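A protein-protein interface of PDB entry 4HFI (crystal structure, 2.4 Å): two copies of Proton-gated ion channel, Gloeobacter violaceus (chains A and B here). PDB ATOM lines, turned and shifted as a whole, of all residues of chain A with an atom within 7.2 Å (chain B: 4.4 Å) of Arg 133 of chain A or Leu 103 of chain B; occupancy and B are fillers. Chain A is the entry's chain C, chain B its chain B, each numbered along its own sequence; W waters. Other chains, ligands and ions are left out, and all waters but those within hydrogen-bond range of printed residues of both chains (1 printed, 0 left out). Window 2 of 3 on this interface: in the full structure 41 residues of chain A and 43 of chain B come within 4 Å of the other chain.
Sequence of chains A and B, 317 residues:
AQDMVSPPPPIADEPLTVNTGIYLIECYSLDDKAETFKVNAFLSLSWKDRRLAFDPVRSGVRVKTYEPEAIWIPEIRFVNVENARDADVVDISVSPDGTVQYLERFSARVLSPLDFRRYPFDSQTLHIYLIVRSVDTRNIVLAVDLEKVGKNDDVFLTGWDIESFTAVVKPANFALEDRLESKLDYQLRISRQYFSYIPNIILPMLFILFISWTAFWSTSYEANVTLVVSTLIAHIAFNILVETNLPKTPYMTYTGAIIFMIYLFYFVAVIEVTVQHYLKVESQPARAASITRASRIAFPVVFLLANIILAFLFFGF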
ATOM      1  N   GLU A  75      -4.456 -11.858  -2.461  1.00  0.00           N
ATOM      2  CA  GLU A  75      -3.368 -12.811  -2.655  1.00  0.00           C
ATOM      3  C   GLU A  75      -3.860 -14.199  -2.265  1.00  0.00           C
ATOM      4  O   GLU A  75      -3.743 -14.608  -1.106  1.00  0.00           O
ATOM      5  CB  GLU A  75      -2.137 -12.420  -1.831  1.00  0.00           C
ATOM      6  CG  GLU A  75      -1.343 -11.251  -2.388  1.00  0.00           C
ATOM      7  CD  GLU A  75      -0.129 -10.882  -1.560  1.00  0.00           C
ATOM      8  OE1 GLU A  75       0.081 -11.508  -0.496  1.00  0.00           O
ATOM      9  OE2 GLU A  75       0.626  -9.977  -1.985  1.00  0.00           O
ATOM     10  N   ILE A  76      -4.456 -14.899  -3.237  1.00  0.00           N
ATOM     11  CA  ILE A  76      -4.985 -16.247  -3.044  1.00  0.00           C
ATOM     12  C   ILE A  76      -3.913 -17.266  -3.424  1.00  0.00           C
ATOM     13  O   ILE A  76      -3.320 -17.172  -4.501  1.00  0.00           O
ATOM     14  CB  ILE A  76      -6.318 -16.450  -3.822  1.00  0.00           C
ATOM     15  CG1 ILE A  76      -7.345 -15.295  -3.581  1.00  0.00           C
ATOM     16  CG2 ILE A  76      -6.924 -17.829  -3.566  1.00  0.00           C
ATOM     17  CD1 ILE A  76      -7.999 -15.164  -2.189  1.00  0.00           C
ATOM     18  N   ARG A  77      -3.642 -18.216  -2.522  1.00  0.00           N
ATOM     19  CA  ARG A  77      -2.642 -19.261  -2.751  1.00  0.00           C
ATOM     20  C   ARG A  77      -3.215 -20.644  -2.480  1.00  0.00           C
ATOM     21  O   ARG A  77      -4.265 -20.783  -1.847  1.00  0.00           O
ATOM     22  CB  ARG A  77      -1.404 -19.039  -1.864  1.00  0.00           C
ATOM     23  CG  ARG A  77      -0.543 -17.852  -2.275  1.00  0.00           C
ATOM     24  CD  ARG A  77       0.649 -17.637  -1.350  1.00  0.00           C
ATOM     25  NE  ARG A  77       0.256 -17.497   0.058  1.00  0.00           N
ATOM     26  CZ  ARG A  77      -0.171 -16.371   0.625  1.00  0.00           C
ATOM     27  NH1 ARG A  77      -0.269 -15.255  -0.090  1.00  0.00           N
ATOM     28  NH2 ARG A  77      -0.509 -16.352   1.906  1.00  0.00           N
ATOM     29  N   ILE A 131      -6.252 -20.843   0.045  1.00  0.00           N
ATOM     30  CA  ILE A 131      -5.913 -20.051   1.225  1.00  0.00           C
ATOM     31  C   ILE A 131      -5.678 -18.555   0.967  1.00  0.00           C
ATOM     32  O   ILE A 131      -5.202 -18.161  -0.104  1.00  0.00           O
ATOM     33  CB  ILE A 131      -4.767 -20.735   2.032  1.00  0.00           C
ATOM     34  CG1 ILE A 131      -4.813 -20.363   3.529  1.00  0.00           C
ATOM     35  CG2 ILE A 131      -3.383 -20.522   1.390  1.00  0.00           C
ATOM     36  CD1 ILE A 131      -4.290 -21.423   4.496  1.00  0.00           C
ATOM     37  N   VAL A 132      -6.028 -17.733   1.968  1.00  0.00           N
ATOM     38  CA  VAL A 132      -5.811 -16.292   1.992  1.00  0.00           C
ATOM     39  C   VAL A 132      -5.319 -15.872   3.378  1.00  0.00           C
ATOM     40  O   VAL A 132      -5.838 -16.350   4.397  1.00  0.00           O
ATOM     41  CB  VAL A 132      -6.995 -15.432   1.456  1.00  0.00           C
ATOM     42  CG1 VAL A 132      -8.153 -15.347   2.456  1.00  0.00           C
ATOM     43  CG2 VAL A 132      -6.518 -14.037   1.044  1.00  0.00           C
ATOM     44  N   ARG A 133      -4.271 -15.037   3.396  1.00  0.00           N
ATOM     45  CA  ARG A 133      -3.695 -14.475   4.609  1.00  0.00           C
ATOM     46  C   ARG A 133      -4.230 -13.037   4.759  1.00  0.00           C
ATOM     47  O   ARG A 133      -4.181 -12.254   3.803  1.00  0.00           O
ATOM     48  CB  ARG A 133      -2.157 -14.518   4.546  1.00  0.00           C
ATOM     49  CG  ARG A 133      -1.457 -13.523   5.471  1.00  0.00           C
ATOM     50  CD  ARG A 133      -0.042 -13.924   5.779  1.00  0.00           C
ATOM     51  NE  ARG A 133      -0.023 -14.950   6.815  1.00  0.00           N
ATOM     52  CZ  ARG A 133       0.512 -14.794   8.018  1.00  0.00           C
ATOM     53  NH1 ARG A 133       0.479 -15.782   8.895  1.00  0.00           N
ATOM     54  NH2 ARG A 133       1.111 -13.655   8.345  1.00  0.00           N
ATOM     55  N   SER A 134      -4.753 -12.709   5.955  1.00  0.00           N
ATOM     56  CA  SER A 134      -5.291 -11.385   6.275  1.00  0.00           C
ATOM     57  C   SER A 134      -4.200 -10.317   6.286  1.00  0.00           C
ATOM     58  O   SER A 134      -3.025 -10.620   6.522  1.00  0.00           O
ATOM     59  CB  SER A 134      -6.006 -11.410   7.622  1.00  0.00           C
ATOM     60  OG  SER A 134      -7.167 -12.221   7.563  1.00  0.00           O
ATOM     61  N   VAL A 135      -4.600  -9.070   6.012  1.00  0.00           N
ATOM     62  CA  VAL A 135      -3.726  -7.897   5.994  1.00  0.00           C
ATOM     63  C   VAL A 135      -3.940  -7.079   7.282  1.00  0.00           C
ATOM     64  O   VAL A 135      -4.926  -7.311   7.991  1.00  0.00           O
ATOM     65  CB  VAL A 135      -3.877  -7.069   4.688  1.00  0.00           C
ATOM     66  CG1 VAL A 135      -3.323  -7.836   3.487  1.00  0.00           C
ATOM     67  CG2 VAL A 135      -5.330  -6.663   4.440  1.00  0.00           C
ATOM     68  N   ARG A 138      -7.343  -5.076   7.270  1.00  0.00           N
ATOM     69  CA  ARG A 138      -8.525  -5.924   7.502  1.00  0.00           C
ATOM     70  C   ARG A 138      -8.359  -7.427   7.265  1.00  0.00           C
ATOM     71  O   ARG A 138      -7.479  -7.862   6.525  1.00  0.00           O
ATOM     72  CB  ARG A 138      -9.819  -5.365   6.867  1.00  0.00           C
ATOM     73  CG  ARG A 138      -9.987  -5.584   5.369  1.00  0.00           C
ATOM     74  CD  ARG A 138     -11.147  -4.750   4.850  1.00  0.00           C
ATOM     75  NE  ARG A 138     -12.455  -5.274   5.252  1.00  0.00           N
ATOM     76  CZ  ARG A 138     -13.541  -5.251   4.484  1.00  0.00           C
ATOM     77  NH1 ARG A 138     -13.491  -4.722   3.266  1.00  0.00           N
ATOM     78  NH2 ARG A 138     -14.684  -5.754   4.926  1.00  0.00           N
ATOM     79  N   ASN A 139      -9.234  -8.211   7.904  1.00  0.00           N
ATOM     80  CA  ASN A 139      -9.275  -9.662   7.804  1.00  0.00           C
ATOM     81  C   ASN A 139      -9.968 -10.106   6.526  1.00  0.00           C
ATOM     82  O   ASN A 139     -11.016  -9.561   6.178  1.00  0.00           O
ATOM     83  CB  ASN A 139      -9.952 -10.262   9.035  1.00  0.00           C
ATOM     84  CG  ASN A 139      -9.164 -10.097  10.318  1.00  0.00           C
ATOM     85  OD1 ASN A 139      -7.973  -9.752  10.329  1.00  0.00           O
ATOM     86  ND2 ASN A 139      -9.814 -10.368  11.437  1.00  0.00           N
ATOM     87  N   ILE A 140      -9.365 -11.077   5.807  1.00  0.00           N
ATOM     88  CA  ILE A 140      -9.924 -11.616   4.563  1.00  0.00           C
ATOM     89  C   ILE A 140     -10.386 -13.062   4.795  1.00  0.00           C
ATOM     90  O   ILE A 140      -9.614 -13.904   5.256  1.00  0.00           O
ATOM     91  CB  ILE A 140      -8.985 -11.461   3.329  1.00  0.00           C
ATOM     92  CG1 ILE A 140      -8.295 -10.074   3.280  1.00  0.00           C
ATOM     93  CG2 ILE A 140      -9.759 -11.727   2.040  1.00  0.00           C
ATOM     94  CD1 ILE A 140      -6.983 -10.044   2.485  1.00  0.00           C
ATOM     95  N   PHE A 174      -8.172 -19.744  11.050  1.00  0.00           N
ATOM     96  CA  PHE A 174      -7.191 -19.977  12.104  1.00  0.00           C
ATOM     97  C   PHE A 174      -6.085 -18.933  12.088  1.00  0.00           C
ATOM     98  O   PHE A 174      -5.848 -18.287  11.063  1.00  0.00           O
ATOM     99  CB  PHE A 174      -6.593 -21.398  11.966  1.00  0.00           C
ATOM    100  CG  PHE A 174      -5.848 -21.660  10.676  1.00  0.00           C
ATOM    101  CD1 PHE A 174      -4.462 -21.591  10.628  1.00  0.00           C
ATOM    102  CD2 PHE A 174      -6.532 -21.991   9.511  1.00  0.00           C
ATOM    103  CE1 PHE A 174      -3.775 -21.823   9.435  1.00  0.00           C
ATOM    104  CE2 PHE A 174      -5.844 -22.219   8.319  1.00  0.00           C
ATOM    105  CZ  PHE A 174      -4.468 -22.139   8.290  1.00  0.00           C
ATOM    106  N   ALA A 175      -5.401 -18.782  13.227  1.00  0.00           N
ATOM    107  CA  ALA A 175      -4.288 -17.856  13.359  1.00  0.00           C
ATOM    108  C   ALA A 175      -2.999 -18.593  13.037  1.00  0.00           C
ATOM    109  O   ALA A 175      -2.766 -19.695  13.538  1.00  0.00           O
ATOM    110  CB  ALA A 175      -4.237 -17.290  14.769  1.00  0.00           C
ATOM    111  N   LEU A 176      -2.176 -17.983  12.190  1.00  0.00           N
ATOM    112  CA  LEU A 176      -0.880 -18.499  11.777  1.00  0.00           C
ATOM    113  C   LEU A 176       0.075 -17.313  11.733  1.00  0.00           C
ATOM    114  O   LEU A 176      -0.173 -16.376  10.972  1.00  0.00           O
ATOM    115  CB  LEU A 176      -0.989 -19.211  10.402  1.00  0.00           C
ATOM    116  CG  LEU A 176       0.313 -19.607   9.668  1.00  0.00           C
ATOM    117  CD1 LEU A 176       1.230 -20.424  10.552  1.00  0.00           C
ATOM    118  CD2 LEU A 176       0.012 -20.360   8.387  1.00  0.00           C
ATOM    119  N   GLU A 177       1.148 -17.359  12.570  1.00  0.00           N
ATOM    120  CA  GLU A 177       2.180 -16.313  12.667  1.00  0.00           C
ATOM    121  C   GLU A 177       1.593 -14.906  12.873  1.00  0.00           C
ATOM    122  O   GLU A 177       1.874 -13.975  12.104  1.00  0.00           O
ATOM    123  CB  GLU A 177       3.169 -16.377  11.486  1.00  0.00           C
ATOM    124  CG  GLU A 177       4.201 -17.488  11.597  1.00  0.00           C
ATOM    125  CD  GLU A 177       5.319 -17.488  10.569  1.00  0.00           C
ATOM    126  OE1 GLU A 177       6.175 -18.396  10.643  1.00  0.00           O
ATOM    127  OE2 GLU A 177       5.366 -16.573   9.713  1.00  0.00           O
ATOM    128  N   ASP A 178       0.745 -14.779  13.905  1.00  0.00           N
ATOM    129  CA  ASP A 178       0.063 -13.563  14.354  1.00  0.00           C
ATOM    130  C   ASP A 178      -0.834 -12.847  13.324  1.00  0.00           C
ATOM    131  O   ASP A 178      -0.979 -11.621  13.384  1.00  0.00           O
ATOM    132  CB  ASP A 178       1.025 -12.617  15.102  1.00  0.00           C
ATOM    133  CG  ASP A 178       1.760 -13.295  16.247  1.00  0.00           C
ATOM    134  OD1 ASP A 178       1.160 -13.444  17.331  1.00  0.00           O
ATOM    135  OD2 ASP A 178       2.941 -13.664  16.061  1.00  0.00           O
ATOM    136  N   ARG A 179      -1.457 -13.621  12.403  1.00  0.00           N
ATOM    137  CA  ARG A 179      -2.408 -13.144  11.390  1.00  0.00           C
ATOM    138  C   ARG A 179      -3.443 -14.215  11.070  1.00  0.00           C
ATOM    139  O   ARG A 179      -3.137 -15.404  11.150  1.00  0.00           O
ATOM    140  CB  ARG A 179      -1.709 -12.740  10.080  1.00  0.00           C
ATOM    141  CG  ARG A 179      -0.889 -11.467  10.149  1.00  0.00           C
ATOM    142  CD  ARG A 179      -1.735 -10.210  10.085  1.00  0.00           C
ATOM    143  NE  ARG A 179      -0.919  -9.002  10.202  1.00  0.00           N
ATOM    144  CZ  ARG A 179      -0.261  -8.448   9.189  1.00  0.00           C
ATOM    145  NH1 ARG A 179       0.463  -7.355   9.381  1.00  0.00           N
ATOM    146  NH2 ARG A 179      -0.315  -8.987   7.977  1.00  0.00           N
ATOM    147  N   LEU A 180      -4.662 -13.796  10.693  1.00  0.00           N
ATOM    148  CA  LEU A 180      -5.722 -14.725  10.325  1.00  0.00           C
ATOM    149  C   LEU A 180      -5.468 -15.325   8.946  1.00  0.00           C
ATOM    150  O   LEU A 180      -4.984 -14.650   8.033  1.00  0.00           O
ATOM    151  CB  LEU A 180      -7.118 -14.066  10.385  1.00  0.00           C
ATOM    152  CG  LEU A 180      -8.316 -14.924   9.907  1.00  0.00           C
ATOM    153  CD1 LEU A 180      -8.778 -15.903  10.978  1.00  0.00           C
ATOM    154  CD2 LEU A 180      -9.466 -14.060   9.445  1.00  0.00           C
ATOM    155  N   GLU A 181      -5.807 -16.608   8.823  1.00  0.00           N
ATOM    156  CA  GLU A 181      -5.713 -17.394   7.610  1.00  0.00           C
ATOM    157  C   GLU A 181      -7.077 -18.060   7.382  1.00  0.00           C
ATOM    158  O   GLU A 181      -7.650 -18.599   8.332  1.00  0.00           O
ATOM    159  CB  GLU A 181      -4.596 -18.429   7.757  1.00  0.00           C
ATOM    160  CG  GLU A 181      -3.780 -18.594   6.495  1.00  0.00           C
ATOM    161  CD  GLU A 181      -2.476 -17.838   6.363  1.00  0.00           C
ATOM    162  OE1 GLU A 181      -1.932 -17.375   7.391  1.00  0.00           O
ATOM    163  OE2 GLU A 181      -1.960 -17.776   5.226  1.00  0.00           O
ATOM    164  N   SER A 182      -7.625 -17.948   6.151  1.00  0.00           N
ATOM    165  CA  SER A 182      -8.918 -18.526   5.763  1.00  0.00           C
ATOM    166  C   SER A 182      -8.675 -19.609   4.708  1.00  0.00           C
ATOM    167  O   SER A 182      -8.216 -19.304   3.603  1.00  0.00           O
ATOM    168  CB  SER A 182      -9.857 -17.442   5.238  1.00  0.00           C
ATOM    169  OG  SER A 182     -11.203 -17.888   5.200  1.00  0.00           O
ATOM    170  N   PHE B  42       7.219 -20.898   4.453  1.00  0.00           N
ATOM    171  CA  PHE B  42       7.179 -19.461   4.649  1.00  0.00           C
ATOM    172  C   PHE B  42       8.532 -19.072   5.194  1.00  0.00           C
ATOM    173  O   PHE B  42       9.036 -19.738   6.105  1.00  0.00           O
ATOM    174  CB  PHE B  42       6.118 -19.063   5.698  1.00  0.00           C
ATOM    175  CG  PHE B  42       4.720 -18.754   5.219  1.00  0.00           C
ATOM    176  CD1 PHE B  42       4.505 -18.128   3.994  1.00  0.00           C
ATOM    177  CD2 PHE B  42       3.621 -19.016   6.026  1.00  0.00           C
ATOM    178  CE1 PHE B  42       3.213 -17.829   3.564  1.00  0.00           C
ATOM    179  CE2 PHE B  42       2.329 -18.703   5.600  1.00  0.00           C
ATOM    180  CZ  PHE B  42       2.135 -18.106   4.375  1.00  0.00           C
ATOM    181  N   LEU B  43       9.132 -18.013   4.643  1.00  0.00           N
ATOM    182  CA  LEU B  43      10.368 -17.437   5.160  1.00  0.00           C
ATOM    183  C   LEU B  43      10.010 -16.034   5.619  1.00  0.00           C
ATOM    184  O   LEU B  43       9.593 -15.200   4.804  1.00  0.00           O
ATOM    185  CB  LEU B  43      11.523 -17.406   4.138  1.00  0.00           C
ATOM    186  CG  LEU B  43      12.759 -16.554   4.543  1.00  0.00           C
ATOM    187  CD1 LEU B  43      13.567 -17.219   5.651  1.00  0.00           C
ATOM    188  CD2 LEU B  43      13.636 -16.253   3.345  1.00  0.00           C
ATOM    189  N   SER B  44      10.121 -15.798   6.932  1.00  0.00           N
ATOM    190  CA  SER B  44       9.833 -14.502   7.523  1.00  0.00           C
ATOM    191  C   SER B  44      11.138 -13.787   7.861  1.00  0.00           C
ATOM    192  O   SER B  44      12.093 -14.425   8.312  1.00  0.00           O
ATOM    193  CB  SER B  44       8.927 -14.641   8.744  1.00  0.00           C
ATOM    194  OG  SER B  44       9.582 -15.238   9.850  1.00  0.00           O
ATOM    195  N   VAL B  89       6.792 -12.969  -2.780  1.00  0.00           N
ATOM    196  CA  VAL B  89       6.578 -12.094  -1.629  1.00  0.00           C
ATOM    197  C   VAL B  89       5.082 -12.064  -1.293  1.00  0.00           C
ATOM    198  O   VAL B  89       4.253 -11.826  -2.174  1.00  0.00           O
ATOM    199  CB  VAL B  89       7.196 -10.677  -1.806  1.00  0.00           C
ATOM    200  CG1 VAL B  89       6.954  -9.811  -0.570  1.00  0.00           C
ATOM    201  CG2 VAL B  89       8.690 -10.758  -2.103  1.00  0.00           C
ATOM    202  N   VAL B  90       4.750 -12.392  -0.035  1.00  0.00           N
ATOM    203  CA  VAL B  90       3.379 -12.384   0.476  1.00  0.00           C
ATOM    204  C   VAL B  90       3.099 -10.987   1.055  1.00  0.00           C
ATOM    205  O   VAL B  90       2.082 -10.381   0.726  1.00  0.00           O
ATOM    206  CB  VAL B  90       3.125 -13.528   1.502  1.00  0.00           C
ATOM    207  CG1 VAL B  90       1.743 -13.417   2.150  1.00  0.00           C
ATOM    208  CG2 VAL B  90       3.303 -14.903   0.859  1.00  0.00           C
ATOM    209  N   ASP B  91       4.016 -10.463   1.888  1.00  0.00           N
ATOM    210  CA  ASP B  91       3.831  -9.155   2.508  1.00  0.00           C
ATOM    211  C   ASP B  91       5.119  -8.494   2.946  1.00  0.00           C
ATOM    212  O   ASP B  91       6.068  -9.171   3.341  1.00  0.00           O
ATOM    213  CB  ASP B  91       2.888  -9.285   3.722  1.00  0.00           C
ATOM    214  CG  ASP B  91       2.256  -7.991   4.213  1.00  0.00           C
ATOM    215  OD1 ASP B  91       2.185  -7.019   3.419  1.00  0.00           O
ATOM    216  OD2 ASP B  91       1.787  -7.965   5.371  1.00  0.00           O
ATOM    217  N   GLN B 101       8.592  -6.028   8.436  1.00  0.00           N
ATOM    218  CA  GLN B 101       8.130  -7.398   8.565  1.00  0.00           C
ATOM    219  C   GLN B 101       7.904  -7.922   7.158  1.00  0.00           C
ATOM    220  O   GLN B 101       6.965  -7.510   6.468  1.00  0.00           O
ATOM    221  CB  GLN B 101       6.891  -7.524   9.463  1.00  0.00           C
ATOM    222  CG  GLN B 101       7.265  -7.618  10.938  1.00  0.00           C
ATOM    223  CD  GLN B 101       6.122  -8.093  11.800  1.00  0.00           C
ATOM    224  OE1 GLN B 101       5.076  -7.441  11.904  1.00  0.00           O
ATOM    225  NE2 GLN B 101       6.311  -9.221  12.471  1.00  0.00           N
ATOM    226  N   TYR B 102       8.845  -8.762   6.711  1.00  0.00           N
ATOM    227  CA  TYR B 102       8.885  -9.374   5.388  1.00  0.00           C
ATOM    228  C   TYR B 102       8.417 -10.816   5.469  1.00  0.00           C
ATOM    229  O   TYR B 102       8.891 -11.576   6.317  1.00  0.00           O
ATOM    230  CB  TYR B 102      10.326  -9.295   4.834  1.00  0.00           C
ATOM    231  CG  TYR B 102      10.563  -9.986   3.507  1.00  0.00           C
ATOM    232  CD1 TYR B 102      10.852 -11.348   3.448  1.00  0.00           C
ATOM    233  CD2 TYR B 102      10.591  -9.263   2.318  1.00  0.00           C
ATOM    234  CE1 TYR B 102      11.110 -11.981   2.235  1.00  0.00           C
ATOM    235  CE2 TYR B 102      10.842  -9.888   1.096  1.00  0.00           C
ATOM    236  CZ  TYR B 102      11.101 -11.249   1.060  1.00  0.00           C
ATOM    237  OH  TYR B 102      11.355 -11.876  -0.137  1.00  0.00           O
ATOM    238  N   LEU B 103       7.511 -11.201   4.562  1.00  0.00           N
ATOM    239  CA  LEU B 103       7.018 -12.566   4.473  1.00  0.00           C
ATOM    240  C   LEU B 103       6.962 -13.044   3.032  1.00  0.00           C
ATOM    241  O   LEU B 103       6.337 -12.413   2.181  1.00  0.00           O
ATOM    242  CB  LEU B 103       5.666 -12.777   5.196  1.00  0.00           C
ATOM    243  CG  LEU B 103       5.163 -14.245   5.273  1.00  0.00           C
ATOM    244  CD1 LEU B 103       6.036 -15.106   6.181  1.00  0.00           C
ATOM    245  CD2 LEU B 103       3.703 -14.310   5.703  1.00  0.00           C
ATOM    246  N   GLU B 104       7.642 -14.156   2.768  1.00  0.00           N
ATOM    247  CA  GLU B 104       7.643 -14.787   1.459  1.00  0.00           C
ATOM    248  C   GLU B 104       7.324 -16.248   1.597  1.00  0.00           C
ATOM    249  O   GLU B 104       7.633 -16.871   2.621  1.00  0.00           O
ATOM    250  CB  GLU B 104       8.984 -14.599   0.715  1.00  0.00           C
ATOM    251  CG  GLU B 104      10.182 -15.292   1.351  1.00  0.00           C
ATOM    252  CD  GLU B 104      11.362 -15.516   0.428  1.00  0.00           C
ATOM    253  OE1 GLU B 104      11.983 -14.519  -0.004  1.00  0.00           O
ATOM    254  OE2 GLU B 104      11.683 -16.695   0.160  1.00  0.00           O
HETATM  255  O   HOH W   1       8.296 -17.935   9.417  1.00  0.00           O
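No position is printed for both chains. Of the 6 pairs that touch across the chains among the printed residues, none has its exchanged pair printed and touching as well.
CG1 of Val 90 of chain B touches NH1 of Arg 77 of chain A, at 3.5 Å. Arg 133 of chain A touches Leu 103 of chain B. Leu 176 of chain A touches Phe 42 of chain B. Leu 103 of chain B touches Glu 177 of chain A.
The backbone carbonyl oxygen (O) of Leu 103 of chain B lies within hydrogen-bond range of the backbone NH (N) of Val 90 of chain B, 2.7 Å away. The backbone NH of Leu 103 of chain B lies within hydrogen-bond range of the backbone carbonyl oxygen of Asp 91 of chain B (2.8 Å). The backbone carbonyl oxygen (O) of Arg 77 of chain A is in hydrogen-bond range of the backbone NH (N) of Ile 131 of chain A (2.7 Å). The guanidinium group of Arg 77 of chain A lies within salt-bridge range of the side-chain carboxylate of Glu 181 of chain A (3.9 Å). OE1 of Glu 181 of chain A lies within salt-bridge range of NE of Arg 133 of chain A, 3.1 Å away. The guanidinium group (NH2) of Arg 179 of chain A is in hydrogen-bond range of the backbone carbonyl oxygen (O) of Ser 134 of chain A (3.5 Å).
Printed residues of chain A that touch a printed residue of chain B: Glu 75, Arg 77, Arg 133, Leu 176, Glu 177 and Arg 179. Hydrophobic or aromatic side chains of chain A that line the printed part of chain B: Leu 176. Of the 10 printed residues of chain B, 4 touch a printed residue of chain A. Hydrophobic or aromatic side chains of chain B within 4 Å of the printed part of chain A: Phe 42, Val 90 and Leu 103. Among the printed residues, 6 pairs touch across the chains. Among the printed residues, Asp or Glu carboxylates within 4 Å of a Lys or Arg side-chain nitrogen of the other chain: Arg 179 of chain A with Asp 91 of chain B.
Arg 133 of chain A touches one residue of chain B. Ala 175 of chain A touches none of the printed residues of chain B. Of the printed residues of chain B, Leu 176 of chain A touches Phe 42. Of the printed residues of chain A, Asp 91 of chain B touches Arg 179 (3.5 Å). Printed residues of chain A within 4 Å of Leu 103 of chain B: Arg 133 (3.8 Å) and Glu 177 (3.9 Å). The nearest residue of chain B that does not touch Arg 133 of chain A is Val 90 of chain B (4.1 Å).
Water W1 bridges OE1 of Glu 177 of chain A (2.5 Å) and OG of Ser 44 of chain B (3.0 Å).
The backbone carbonyl oxygen (O) of Val 90 of chain B sits close to the side-chain carboxylate (OE1) of Glu 75 of chain A (2.6 Å). The side-chain carboxylate (OD2) of Asp 91 of chain B is in salt-bridge range of the guanidinium group (NH2) of Arg 179 of chain A.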
